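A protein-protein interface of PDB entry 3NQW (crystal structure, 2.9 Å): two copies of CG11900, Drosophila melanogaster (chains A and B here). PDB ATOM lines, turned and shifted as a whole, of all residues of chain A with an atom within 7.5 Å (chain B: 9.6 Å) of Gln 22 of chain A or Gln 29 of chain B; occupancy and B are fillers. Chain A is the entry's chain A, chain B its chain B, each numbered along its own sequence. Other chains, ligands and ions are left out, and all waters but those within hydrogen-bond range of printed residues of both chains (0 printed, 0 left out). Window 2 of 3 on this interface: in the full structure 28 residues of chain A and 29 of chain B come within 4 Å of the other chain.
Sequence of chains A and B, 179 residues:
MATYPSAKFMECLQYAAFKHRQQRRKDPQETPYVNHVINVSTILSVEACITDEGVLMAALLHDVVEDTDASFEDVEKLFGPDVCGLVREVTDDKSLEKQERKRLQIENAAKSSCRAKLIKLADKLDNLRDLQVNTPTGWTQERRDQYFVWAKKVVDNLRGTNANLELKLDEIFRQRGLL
The side-chain amide oxygen (OD1) of Asn 35 of chain B lies close to the backbone carbonyl oxygen (O) of Ala 17 of chain A, at 3.4 Å.
The side-chain amide nitrogen (NE2) of Gln 22 of chain A sits at hydrogen-bond distance from the side-chain amide oxygen (OE1) of Gln 29 of chain B (3.3 Å).
The side-chain amide oxygen (OE1) of Gln 29 of chain B sits at hydrogen-bond distance from the guanidinium group (NE) of Arg 21 of chain A, 3.2 Å away.
The guanidinium group (NH2) of Arg 24 of chain A sits close to the guanidinium group (NE) of Arg 24 of chain B (3.5 Å).
The guanidinium group (NH2) of Arg 24 of chain A lies within hydrogen-bond range of the backbone carbonyl oxygen (O) of Glu 30 of chain B (3.1 Å).
The backbone carbonyl oxygen (O) of Thr 31 of chain B sits at hydrogen-bond distance from the backbone NH (N) of Arg 25 of chain B.
The backbone carbonyl oxygen (O) of Arg 21 of chain A is in hydrogen-bond range of the guanidinium group (NH1) of Arg 24 of chain A, 2.9 Å away.
The side-chain carboxylate (OD2) of Asp 27 of chain B sits at hydrogen-bond distance from the backbone NH (N) of Glu 30 of chain B, 3.4 Å away.
NE of Arg 25 of chain A lies within hydrogen-bond range of O of Pro 32 of chain A (3.4 Å).
NH2 of Arg 21 of chain A lies within hydrogen-bond range of O of Phe 18 of chain A (2.6 Å).
OD1 of Asp 27 of chain B lies within hydrogen-bond range of OG1 of Thr 31 of chain B (2.9 Å).
Arg 21 of chain A touches Thr 31 of chain B.
Arg 21 of chain A touches Pro 32 of chain B (O to CD, 3.0 Å).
Arg 21 of chain A touches Asn 35 of chain B (CB to ND2, 3.6 Å).
Arg 24 of chain A touches Pro 32 of chain B.
CD of Pro 32 of chain A touches NH2 of Arg 24 of chain B (3.5 Å).
Pro 32 of chain A touches Pro 32 of chain B (CB to CG, 3.4 Å).
Arg 21 of chain A touches four residues of chain B.
Gln 22 of chain A touches just one residue of chain B: Gln 29 (3.3 Å).
Printed residues of chain B within 4 Å of Arg 24 of chain A: Arg 24 (3.5 Å), Glu 30 (3.1 Å) and Pro 32 (3.6 Å).
Thr 68 of chain A touches none of the printed residues of chain B.
Of the printed residues of chain A, Glu 30 of chain B touches Arg 24.
Printed residues of chain A within 4 Å of Thr 31 of chain B: Arg 21 (3.8 Å).
Of the printed residues of chain A, Pro 32 of chain B touches Arg 21 (3.0 Å), Arg 24 (3.6 Å) and Pro 32 (3.4 Å).
Of the printed residues of chain A, Asn 35 of chain B touches Ala 17 (3.4 Å) and Arg 21 (3.6 Å).
Pro 136 of chain B touches none of the printed residues of chain A.
The nearest residue of chain B that does not touch Gln 22 of chain A is Pro 32 of chain B (5.3 Å).
The nearest residue of chain A that does not touch Gln 29 of chain B is Arg 24 of chain A (5.1 Å).
The nearest printed residue of chain B that does not touch Ala 17 of chain A is Pro 32 of chain B (6.0 Å).
Printed residues of chain A that touch a printed residue of chain B: Ala 17, Arg 21, Gln 22, Arg 24 and Pro 32.
Hydrophobic or aromatic side chains of chain A within 4 Å of the printed part of chain B: Ala 17 and Pro 32.
Printed residues of chain B that touch a printed residue of chain A: Arg 24, Gln 29, Glu 30, Thr 31, Pro 32 and Asn 35.
Arg 24 of chain A touches its own counterpart, Arg 24 of chain B.
Arg 24 of chain A touches Pro 32 of chain B, and with the chains exchanged Pro 32 of chain A touches Arg 24 of chain B.
Pro 32 of chain B touches its own counterpart, Pro 32 of chain A.
Positions printed for both chains: 24, 25 and 32.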
ATOM      1  N   ALA A  17      28.761  18.585 -10.408  1.00  0.00           N
ATOM      2  CA  ALA A  17      28.233  19.125  -9.151  1.00  0.00           C
ATOM      3  C   ALA A  17      26.712  19.043  -8.988  1.00  0.00           C
ATOM      4  O   ALA A  17      26.196  18.948  -7.869  1.00  0.00           O
ATOM      5  CB  ALA A  17      28.670  20.580  -9.014  1.00  0.00           C
ATOM      6  N   PHE A  18      26.005  19.104 -10.112  1.00  0.00           N
ATOM      7  CA  PHE A  18      24.552  19.060 -10.127  1.00  0.00           C
ATOM      8  C   PHE A  18      23.990  17.652 -10.000  1.00  0.00           C
ATOM      9  O   PHE A  18      23.152  17.379  -9.144  1.00  0.00           O
ATOM     10  CB  PHE A  18      24.031  19.671 -11.420  1.00  0.00           C
ATOM     11  CG  PHE A  18      22.552  19.654 -11.516  1.00  0.00           C
ATOM     12  CD1 PHE A  18      21.792  20.347 -10.585  1.00  0.00           C
ATOM     13  CD2 PHE A  18      21.908  18.906 -12.495  1.00  0.00           C
ATOM     14  CE1 PHE A  18      20.403  20.296 -10.618  1.00  0.00           C
ATOM     15  CE2 PHE A  18      20.508  18.845 -12.543  1.00  0.00           C
ATOM     16  CZ  PHE A  18      19.758  19.543 -11.601  1.00  0.00           C
ATOM     17  N   LYS A  19      24.455  16.772 -10.879  1.00  0.00           N
ATOM     18  CA  LYS A  19      24.019  15.383 -10.912  1.00  0.00           C
ATOM     19  C   LYS A  19      24.325  14.676  -9.582  1.00  0.00           C
ATOM     20  O   LYS A  19      23.541  13.851  -9.106  1.00  0.00           O
ATOM     21  CB  LYS A  19      24.715  14.655 -12.072  1.00  0.00           C
ATOM     22  CG  LYS A  19      24.522  15.280 -13.463  1.00  0.00           C
ATOM     23  CD  LYS A  19      23.307  14.736 -14.212  1.00  0.00           C
ATOM     24  CE  LYS A  19      21.991  15.284 -13.702  1.00  0.00           C
ATOM     25  NZ  LYS A  19      20.830  14.789 -14.503  1.00  0.00           N
ATOM     26  N   HIS A  20      25.466  15.004  -8.983  1.00  0.00           N
ATOM     27  CA  HIS A  20      25.856  14.402  -7.712  1.00  0.00           C
ATOM     28  C   HIS A  20      25.220  15.107  -6.498  1.00  0.00           C
ATOM     29  O   HIS A  20      25.189  14.541  -5.415  1.00  0.00           O
ATOM     30  CB  HIS A  20      27.386  14.434  -7.554  1.00  0.00           C
ATOM     31  CG  HIS A  20      28.123  13.458  -8.418  1.00  0.00           C
ATOM     32  ND1 HIS A  20      28.070  12.092  -8.216  1.00  0.00           N
ATOM     33  CD2 HIS A  20      28.976  13.645  -9.455  1.00  0.00           C
ATOM     34  CE1 HIS A  20      28.858  11.488  -9.083  1.00  0.00           C
ATOM     35  NE2 HIS A  20      29.423  12.409  -9.850  1.00  0.00           N
ATOM     36  N   ARG A  21      24.707  16.324  -6.684  1.00  0.00           N
ATOM     37  CA  ARG A  21      24.123  17.122  -5.604  1.00  0.00           C
ATOM     38  C   ARG A  21      23.531  16.406  -4.386  1.00  0.00           C
ATOM     39  O   ARG A  21      23.675  16.885  -3.253  1.00  0.00           O
ATOM     40  CB  ARG A  21      23.082  18.089  -6.165  1.00  0.00           C
ATOM     41  CG  ARG A  21      21.799  17.453  -6.654  1.00  0.00           C
ATOM     42  CD  ARG A  21      20.815  18.543  -7.070  1.00  0.00           C
ATOM     43  NE  ARG A  21      19.578  18.033  -7.672  1.00  0.00           N
ATOM     44  CZ  ARG A  21      19.523  17.209  -8.716  1.00  0.00           C
ATOM     45  NH1 ARG A  21      18.349  16.811  -9.184  1.00  0.00           N
ATOM     46  NH2 ARG A  21      20.638  16.776  -9.286  1.00  0.00           N
ATOM     47  N   GLN A  22      22.871  15.269  -4.614  1.00  0.00           N
ATOM     48  CA  GLN A  22      22.235  14.480  -3.538  1.00  0.00           C
ATOM     49  C   GLN A  22      23.128  13.375  -2.971  1.00  0.00           C
ATOM     50  O   GLN A  22      22.919  12.907  -1.848  1.00  0.00           O
ATOM     51  CB  GLN A  22      20.926  13.849  -4.047  1.00  0.00           C
ATOM     52  CG  GLN A  22      19.776  14.831  -4.287  1.00  0.00           C
ATOM     53  CD  GLN A  22      18.641  14.221  -5.105  1.00  0.00           C
ATOM     54  OE1 GLN A  22      18.152  13.131  -4.796  1.00  0.00           O
ATOM     55  NE2 GLN A  22      18.214  14.927  -6.153  1.00  0.00           N
ATOM     56  N   GLN A  23      24.132  12.977  -3.747  1.00  0.00           N
ATOM     57  CA  GLN A  23      25.046  11.914  -3.344  1.00  0.00           C
ATOM     58  C   GLN A  23      26.054  12.358  -2.296  1.00  0.00           C
ATOM     59  O   GLN A  23      26.583  13.464  -2.360  1.00  0.00           O
ATOM     60  CB  GLN A  23      25.764  11.382  -4.577  1.00  0.00           C
ATOM     61  CG  GLN A  23      26.537  10.108  -4.357  1.00  0.00           C
ATOM     62  CD  GLN A  23      26.975   9.493  -5.668  1.00  0.00           C
ATOM     63  OE1 GLN A  23      27.484  10.182  -6.553  1.00  0.00           O
ATOM     64  NE2 GLN A  23      26.777   8.191  -5.804  1.00  0.00           N
ATOM     65  N   ARG A  24      26.322  11.482  -1.338  1.00  0.00           N
ATOM     66  CA  ARG A  24      27.261  11.793  -0.271  1.00  0.00           C
ATOM     67  C   ARG A  24      28.280  10.661  -0.074  1.00  0.00           C
ATOM     68  O   ARG A  24      28.001   9.504  -0.388  1.00  0.00           O
ATOM     69  CB  ARG A  24      26.487  12.040   1.024  1.00  0.00           C
ATOM     70  CG  ARG A  24      25.483  13.189   0.941  1.00  0.00           C
ATOM     71  CD  ARG A  24      26.125  14.525   1.266  1.00  0.00           C
ATOM     72  NE  ARG A  24      25.129  15.574   1.423  1.00  0.00           N
ATOM     73  CZ  ARG A  24      24.483  16.157   0.417  1.00  0.00           C
ATOM     74  NH1 ARG A  24      24.731  15.795  -0.832  1.00  0.00           N
ATOM     75  NH2 ARG A  24      23.579  17.103   0.658  1.00  0.00           N
ATOM     76  N   ARG A  25      29.462  11.002   0.439  1.00  0.00           N
ATOM     77  CA  ARG A  25      30.506  10.009   0.667  1.00  0.00           C
ATOM     78  C   ARG A  25      30.241   9.206   1.941  1.00  0.00           C
ATOM     79  O   ARG A  25      29.522   9.653   2.835  1.00  0.00           O
ATOM     80  CB  ARG A  25      31.892  10.684   0.725  1.00  0.00           C
ATOM     81  CG  ARG A  25      32.410  11.155  -0.639  1.00  0.00           C
ATOM     82  CD  ARG A  25      33.784  11.826  -0.558  1.00  0.00           C
ATOM     83  NE  ARG A  25      33.760  13.072   0.214  1.00  0.00           N
ATOM     84  CZ  ARG A  25      34.749  13.967   0.237  1.00  0.00           C
ATOM     85  NH1 ARG A  25      35.853  13.764  -0.472  1.00  0.00           N
ATOM     86  NH2 ARG A  25      34.634  15.068   0.970  1.00  0.00           N
ATOM     87  N   PRO A  32      29.723  15.773   0.999  1.00  0.00           N
ATOM     88  CA  PRO A  32      29.215  15.665  -0.377  1.00  0.00           C
ATOM     89  C   PRO A  32      30.090  14.868  -1.357  1.00  0.00           C
ATOM     90  O   PRO A  32      31.307  14.953  -1.305  1.00  0.00           O
ATOM     91  CB  PRO A  32      29.030  17.134  -0.799  1.00  0.00           C
ATOM     92  CG  PRO A  32      29.953  17.907   0.109  1.00  0.00           C
ATOM     93  CD  PRO A  32      29.811  17.187   1.413  1.00  0.00           C
ATOM     94  N   TYR A  33      29.466  14.099  -2.245  1.00  0.00           N
ATOM     95  CA  TYR A  33      30.232  13.294  -3.184  1.00  0.00           C
ATOM     96  C   TYR A  33      30.940  14.138  -4.230  1.00  0.00           C
ATOM     97  O   TYR A  33      31.936  13.714  -4.814  1.00  0.00           O
ATOM     98  CB  TYR A  33      29.345  12.243  -3.870  1.00  0.00           C
ATOM     99  CG  TYR A  33      30.131  11.055  -4.397  1.00  0.00           C
ATOM    100  CD1 TYR A  33      30.873  11.148  -5.570  1.00  0.00           C
ATOM    101  CD2 TYR A  33      30.172   9.849  -3.691  1.00  0.00           C
ATOM    102  CE1 TYR A  33      31.635  10.077  -6.031  1.00  0.00           C
ATOM    103  CE2 TYR A  33      30.937   8.768  -4.151  1.00  0.00           C
ATOM    104  CZ  TYR A  33      31.664   8.897  -5.323  1.00  0.00           C
ATOM    105  OH  TYR A  33      32.434   7.859  -5.801  1.00  0.00           O
ATOM    106  N   VAL A  34      30.432  15.335  -4.474  1.00  0.00           N
ATOM    107  CA  VAL A  34      31.054  16.224  -5.451  1.00  0.00           C
ATOM    108  C   VAL A  34      32.515  16.457  -5.076  1.00  0.00           C
ATOM    109  O   VAL A  34      33.353  16.672  -5.946  1.00  0.00           O
ATOM    110  CB  VAL A  34      30.338  17.597  -5.502  1.00  0.00           C
ATOM    111  CG1 VAL A  34      30.923  18.439  -6.634  1.00  0.00           C
ATOM    112  CG2 VAL A  34      28.817  17.399  -5.686  1.00  0.00           C
ATOM    113  N   THR A  68      24.991   8.690 -10.768  1.00  0.00           N
ATOM    114  CA  THR A  68      23.861   9.587 -10.997  1.00  0.00           C
ATOM    115  C   THR A  68      22.929   9.063 -12.099  1.00  0.00           C
ATOM    116  O   THR A  68      23.092   7.941 -12.590  1.00  0.00           O
ATOM    117  CB  THR A  68      24.344  10.990 -11.409  1.00  0.00           C
ATOM    118  OG1 THR A  68      25.017  10.914 -12.672  1.00  0.00           O
ATOM    119  CG2 THR A  68      25.296  11.550 -10.369  1.00  0.00           C
ATOM    120  N   ASP A  69      21.943   9.875 -12.476  1.00  0.00           N
ATOM    121  CA  ASP A  69      21.011   9.493 -13.525  1.00  0.00           C
ATOM    122  C   ASP A  69      21.437  10.074 -14.872  1.00  0.00           C
ATOM    123  O   ASP A  69      20.610  10.355 -15.726  1.00  0.00           O
ATOM    124  CB  ASP A  69      19.573   9.926 -13.173  1.00  0.00           C
ATOM    125  CG  ASP A  69      19.355  11.433 -13.261  1.00  0.00           C
ATOM    126  OD1 ASP A  69      19.880  12.176 -12.398  1.00  0.00           O
ATOM    127  OD2 ASP A  69      18.639  11.879 -14.192  1.00  0.00           O
ATOM    128  N   ARG B  24      25.838  23.809   3.679  1.00  0.00           N
ATOM    129  CA  ARG B  24      24.838  23.444   2.684  1.00  0.00           C
ATOM    130  C   ARG B  24      23.960  24.641   2.320  1.00  0.00           C
ATOM    131  O   ARG B  24      23.822  25.584   3.102  1.00  0.00           O
ATOM    132  CB  ARG B  24      23.955  22.310   3.220  1.00  0.00           C
ATOM    133  CG  ARG B  24      24.708  21.053   3.651  1.00  0.00           C
ATOM    134  CD  ARG B  24      24.913  20.073   2.511  1.00  0.00           C
ATOM    135  NE  ARG B  24      25.478  18.813   2.986  1.00  0.00           N
ATOM    136  CZ  ARG B  24      26.757  18.625   3.295  1.00  0.00           C
ATOM    137  NH1 ARG B  24      27.629  19.620   3.176  1.00  0.00           N
ATOM    138  NH2 ARG B  24      27.163  17.438   3.729  1.00  0.00           N
ATOM    139  N   ARG B  25      23.378  24.597   1.122  1.00  0.00           N
ATOM    140  CA  ARG B  25      22.496  25.658   0.663  1.00  0.00           C
ATOM    141  C   ARG B  25      21.148  25.445   1.340  1.00  0.00           C
ATOM    142  O   ARG B  25      20.682  24.309   1.487  1.00  0.00           O
ATOM    143  CB  ARG B  25      22.326  25.628  -0.866  1.00  0.00           C
ATOM    144  CG  ARG B  25      23.601  25.901  -1.657  1.00  0.00           C
ATOM    145  CD  ARG B  25      23.342  26.043  -3.166  1.00  0.00           C
ATOM    146  NE  ARG B  25      22.732  24.851  -3.758  1.00  0.00           N
ATOM    147  CZ  ARG B  25      22.630  24.623  -5.067  1.00  0.00           C
ATOM    148  NH1 ARG B  25      23.099  25.507  -5.940  1.00  0.00           N
ATOM    149  NH2 ARG B  25      22.056  23.509  -5.507  1.00  0.00           N
ATOM    150  N   LYS B  26      20.527  26.547   1.752  1.00  0.00           N
ATOM    151  CA  LYS B  26      19.246  26.508   2.442  1.00  0.00           C
ATOM    152  C   LYS B  26      18.062  26.295   1.496  1.00  0.00           C
ATOM    153  O   LYS B  26      17.315  27.228   1.196  1.00  0.00           O
ATOM    154  CB  LYS B  26      19.062  27.803   3.251  1.00  0.00           C
ATOM    155  CG  LYS B  26      20.237  28.137   4.184  1.00  0.00           C
ATOM    156  CD  LYS B  26      20.666  26.942   5.060  1.00  0.00           C
ATOM    157  CE  LYS B  26      22.036  27.168   5.722  1.00  0.00           C
ATOM    158  NZ  LYS B  26      22.581  25.969   6.442  1.00  0.00           N
ATOM    159  N   ASP B  27      17.909  25.061   1.019  1.00  0.00           N
ATOM    160  CA  ASP B  27      16.799  24.700   0.138  1.00  0.00           C
ATOM    161  C   ASP B  27      16.155  23.403   0.662  1.00  0.00           C
ATOM    162  O   ASP B  27      16.640  22.804   1.631  1.00  0.00           O
ATOM    163  CB  ASP B  27      17.282  24.540  -1.329  1.00  0.00           C
ATOM    164  CG  ASP B  27      18.344  23.454  -1.506  1.00  0.00           C
ATOM    165  OD1 ASP B  27      19.421  23.549  -0.899  1.00  0.00           O
ATOM    166  OD2 ASP B  27      18.101  22.504  -2.269  1.00  0.00           O
ATOM    167  N   PRO B  28      15.036  22.972   0.053  1.00  0.00           N
ATOM    168  CA  PRO B  28      14.392  21.740   0.519  1.00  0.00           C
ATOM    169  C   PRO B  28      15.358  20.560   0.488  1.00  0.00           C
ATOM    170  O   PRO B  28      15.561  19.878   1.491  1.00  0.00           O
ATOM    171  CB  PRO B  28      13.233  21.559  -0.461  1.00  0.00           C
ATOM    172  CG  PRO B  28      12.873  22.954  -0.819  1.00  0.00           C
ATOM    173  CD  PRO B  28      14.227  23.625  -0.995  1.00  0.00           C
ATOM    174  N   GLN B  29      15.958  20.331  -0.671  1.00  0.00           N
ATOM    175  CA  GLN B  29      16.889  19.223  -0.825  1.00  0.00           C
ATOM    176  C   GLN B  29      18.083  19.258   0.136  1.00  0.00           C
ATOM    177  O   GLN B  29      18.560  18.209   0.565  1.00  0.00           O
ATOM    178  CB  GLN B  29      17.394  19.172  -2.268  1.00  0.00           C
ATOM    179  CG  GLN B  29      16.327  18.846  -3.305  1.00  0.00           C
ATOM    180  CD  GLN B  29      16.898  18.755  -4.710  1.00  0.00           C
ATOM    181  OE1 GLN B  29      17.833  17.990  -4.960  1.00  0.00           O
ATOM    182  NE2 GLN B  29      16.340  19.537  -5.637  1.00  0.00           N
ATOM    183  N   GLU B  30      18.535  20.468   0.480  1.00  0.00           N
ATOM    184  CA  GLU B  30      19.699  20.731   1.359  1.00  0.00           C
ATOM    185  C   GLU B  30      20.982  20.375   0.614  1.00  0.00           C
ATOM    186  O   GLU B  30      21.864  19.691   1.142  1.00  0.00           O
ATOM    187  CB  GLU B  30      19.652  19.917   2.647  1.00  0.00           C
ATOM    188  CG  GLU B  30      18.526  20.260   3.595  1.00  0.00           C
ATOM    189  CD  GLU B  30      18.502  19.313   4.780  1.00  0.00           C
ATOM    190  OE1 GLU B  30      19.477  19.334   5.566  1.00  0.00           O
ATOM    191  OE2 GLU B  30      17.523  18.541   4.913  1.00  0.00           O
ATOM    192  N   THR B  31      21.064  20.869  -0.618  1.00  0.00           N
ATOM    193  CA  THR B  31      22.195  20.634  -1.508  1.00  0.00           C
ATOM    194  C   THR B  31      23.484  21.288  -0.997  1.00  0.00           C
ATOM    195  O   THR B  31      23.437  22.354  -0.380  1.00  0.00           O
ATOM    196  CB  THR B  31      21.841  21.115  -2.948  1.00  0.00           C
ATOM    197  OG1 THR B  31      21.166  22.372  -2.873  1.00  0.00           O
ATOM    198  CG2 THR B  31      20.908  20.113  -3.635  1.00  0.00           C
ATOM    199  N   PRO B  32      24.656  20.637  -1.227  1.00  0.00           N
ATOM    200  CA  PRO B  32      25.948  21.174  -0.775  1.00  0.00           C
ATOM    201  C   PRO B  32      26.105  22.639  -1.137  1.00  0.00           C
ATOM    202  O   PRO B  32      25.629  23.066  -2.178  1.00  0.00           O
ATOM    203  CB  PRO B  32      26.955  20.292  -1.506  1.00  0.00           C
ATOM    204  CG  PRO B  32      26.240  18.988  -1.606  1.00  0.00           C
ATOM    205  CD  PRO B  32      24.867  19.405  -2.019  1.00  0.00           C
ATOM    206  N   ASN B  35      28.091  23.781  -4.377  1.00  0.00           N
ATOM    207  CA  ASN B  35      27.421  23.935  -5.659  1.00  0.00           C
ATOM    208  C   ASN B  35      27.299  25.418  -5.976  1.00  0.00           C
ATOM    209  O   ASN B  35      27.647  25.875  -7.069  1.00  0.00           O
ATOM    210  CB  ASN B  35      26.051  23.258  -5.633  1.00  0.00           C
ATOM    211  CG  ASN B  35      26.161  21.755  -5.523  1.00  0.00           C
ATOM    212  OD1 ASN B  35      27.260  21.200  -5.537  1.00  0.00           O
ATOM    213  ND2 ASN B  35      25.021  21.082  -5.412  1.00  0.00           N
ATOM    214  N   ASP B 130      18.187  30.786  -7.881  1.00  0.00           N
ATOM    215  CA  ASP B 130      17.863  29.762  -6.907  1.00  0.00           C
ATOM    216  C   ASP B 130      16.697  30.142  -5.989  1.00  0.00           C
ATOM    217  O   ASP B 130      16.048  29.273  -5.407  1.00  0.00           O
ATOM    218  CB  ASP B 130      19.125  29.463  -6.095  1.00  0.00           C
ATOM    219  CG  ASP B 130      19.056  28.147  -5.363  1.00  0.00           C
ATOM    220  OD1 ASP B 130      20.096  27.738  -4.807  1.00  0.00           O
ATOM    221  OD2 ASP B 130      17.974  27.518  -5.332  1.00  0.00           O
ATOM    222  N   ASN B 134      11.504  28.532  -5.407  1.00  0.00           N
ATOM    223  CA  ASN B 134      12.076  27.784  -4.288  1.00  0.00           C
ATOM    224  C   ASN B 134      12.374  28.722  -3.133  1.00  0.00           C
ATOM    225  O   ASN B 134      13.268  29.561  -3.209  1.00  0.00           O
ATOM    226  CB  ASN B 134      13.355  27.092  -4.741  1.00  0.00           C
ATOM    227  CG  ASN B 134      13.297  26.685  -6.193  1.00  0.00           C
ATOM    228  OD1 ASN B 134      13.229  27.534  -7.089  1.00  0.00           O
ATOM    229  ND2 ASN B 134      13.308  25.384  -6.439  1.00  0.00           N
ATOM    230  N   THR B 135      11.614  28.575  -2.061  1.00  0.00           N
ATOM    231  CA  THR B 135      11.793  29.423  -0.903  1.00  0.00           C
ATOM    232  C   THR B 135      12.678  28.764   0.135  1.00  0.00           C
ATOM    233  O   THR B 135      12.550  27.574   0.424  1.00  0.00           O
ATOM    234  CB  THR B 135      10.451  29.761  -0.255  1.00  0.00           C
ATOM    235  OG1 THR B 135       9.646  30.503  -1.178  1.00  0.00           O
ATOM    236  CG2 THR B 135      10.661  30.580   0.995  1.00  0.00           C
ATOM    237  N   PRO B 136      13.595  29.544   0.717  1.00  0.00           N
ATOM    238  CA  PRO B 136      14.511  29.031   1.734  1.00  0.00           C
ATOM    239  C   PRO B 136      13.788  28.324   2.874  1.00  0.00           C
ATOM    240  O   PRO B 136      12.568  28.429   3.019  1.00  0.00           O
ATOM    241  CB  PRO B 136      15.241  30.283   2.189  1.00  0.00           C
ATOM    242  CG  PRO B 136      15.326  31.076   0.921  1.00  0.00           C
ATOM    243  CD  PRO B 136      13.934  30.934   0.362  1.00  0.00           C
ATOM    244  N   THR B 137      14.558  27.592   3.672  1.00  0.00           N
ATOM    245  CA  THR B 137      14.029  26.842   4.805  1.00  0.00           C
ATOM    246  C   THR B 137      13.424  27.806   5.826  1.00  0.00           C
ATOM    247  O   THR B 137      14.090  28.733   6.286  1.00  0.00           O
ATOM    248  CB  THR B 137      15.152  26.008   5.475  1.00  0.00           C
ATOM    249  OG1 THR B 137      15.857  25.267   4.470  1.00  0.00           O
ATOM    250  CG2 THR B 137      14.574  25.036   6.494  1.00  0.00           C
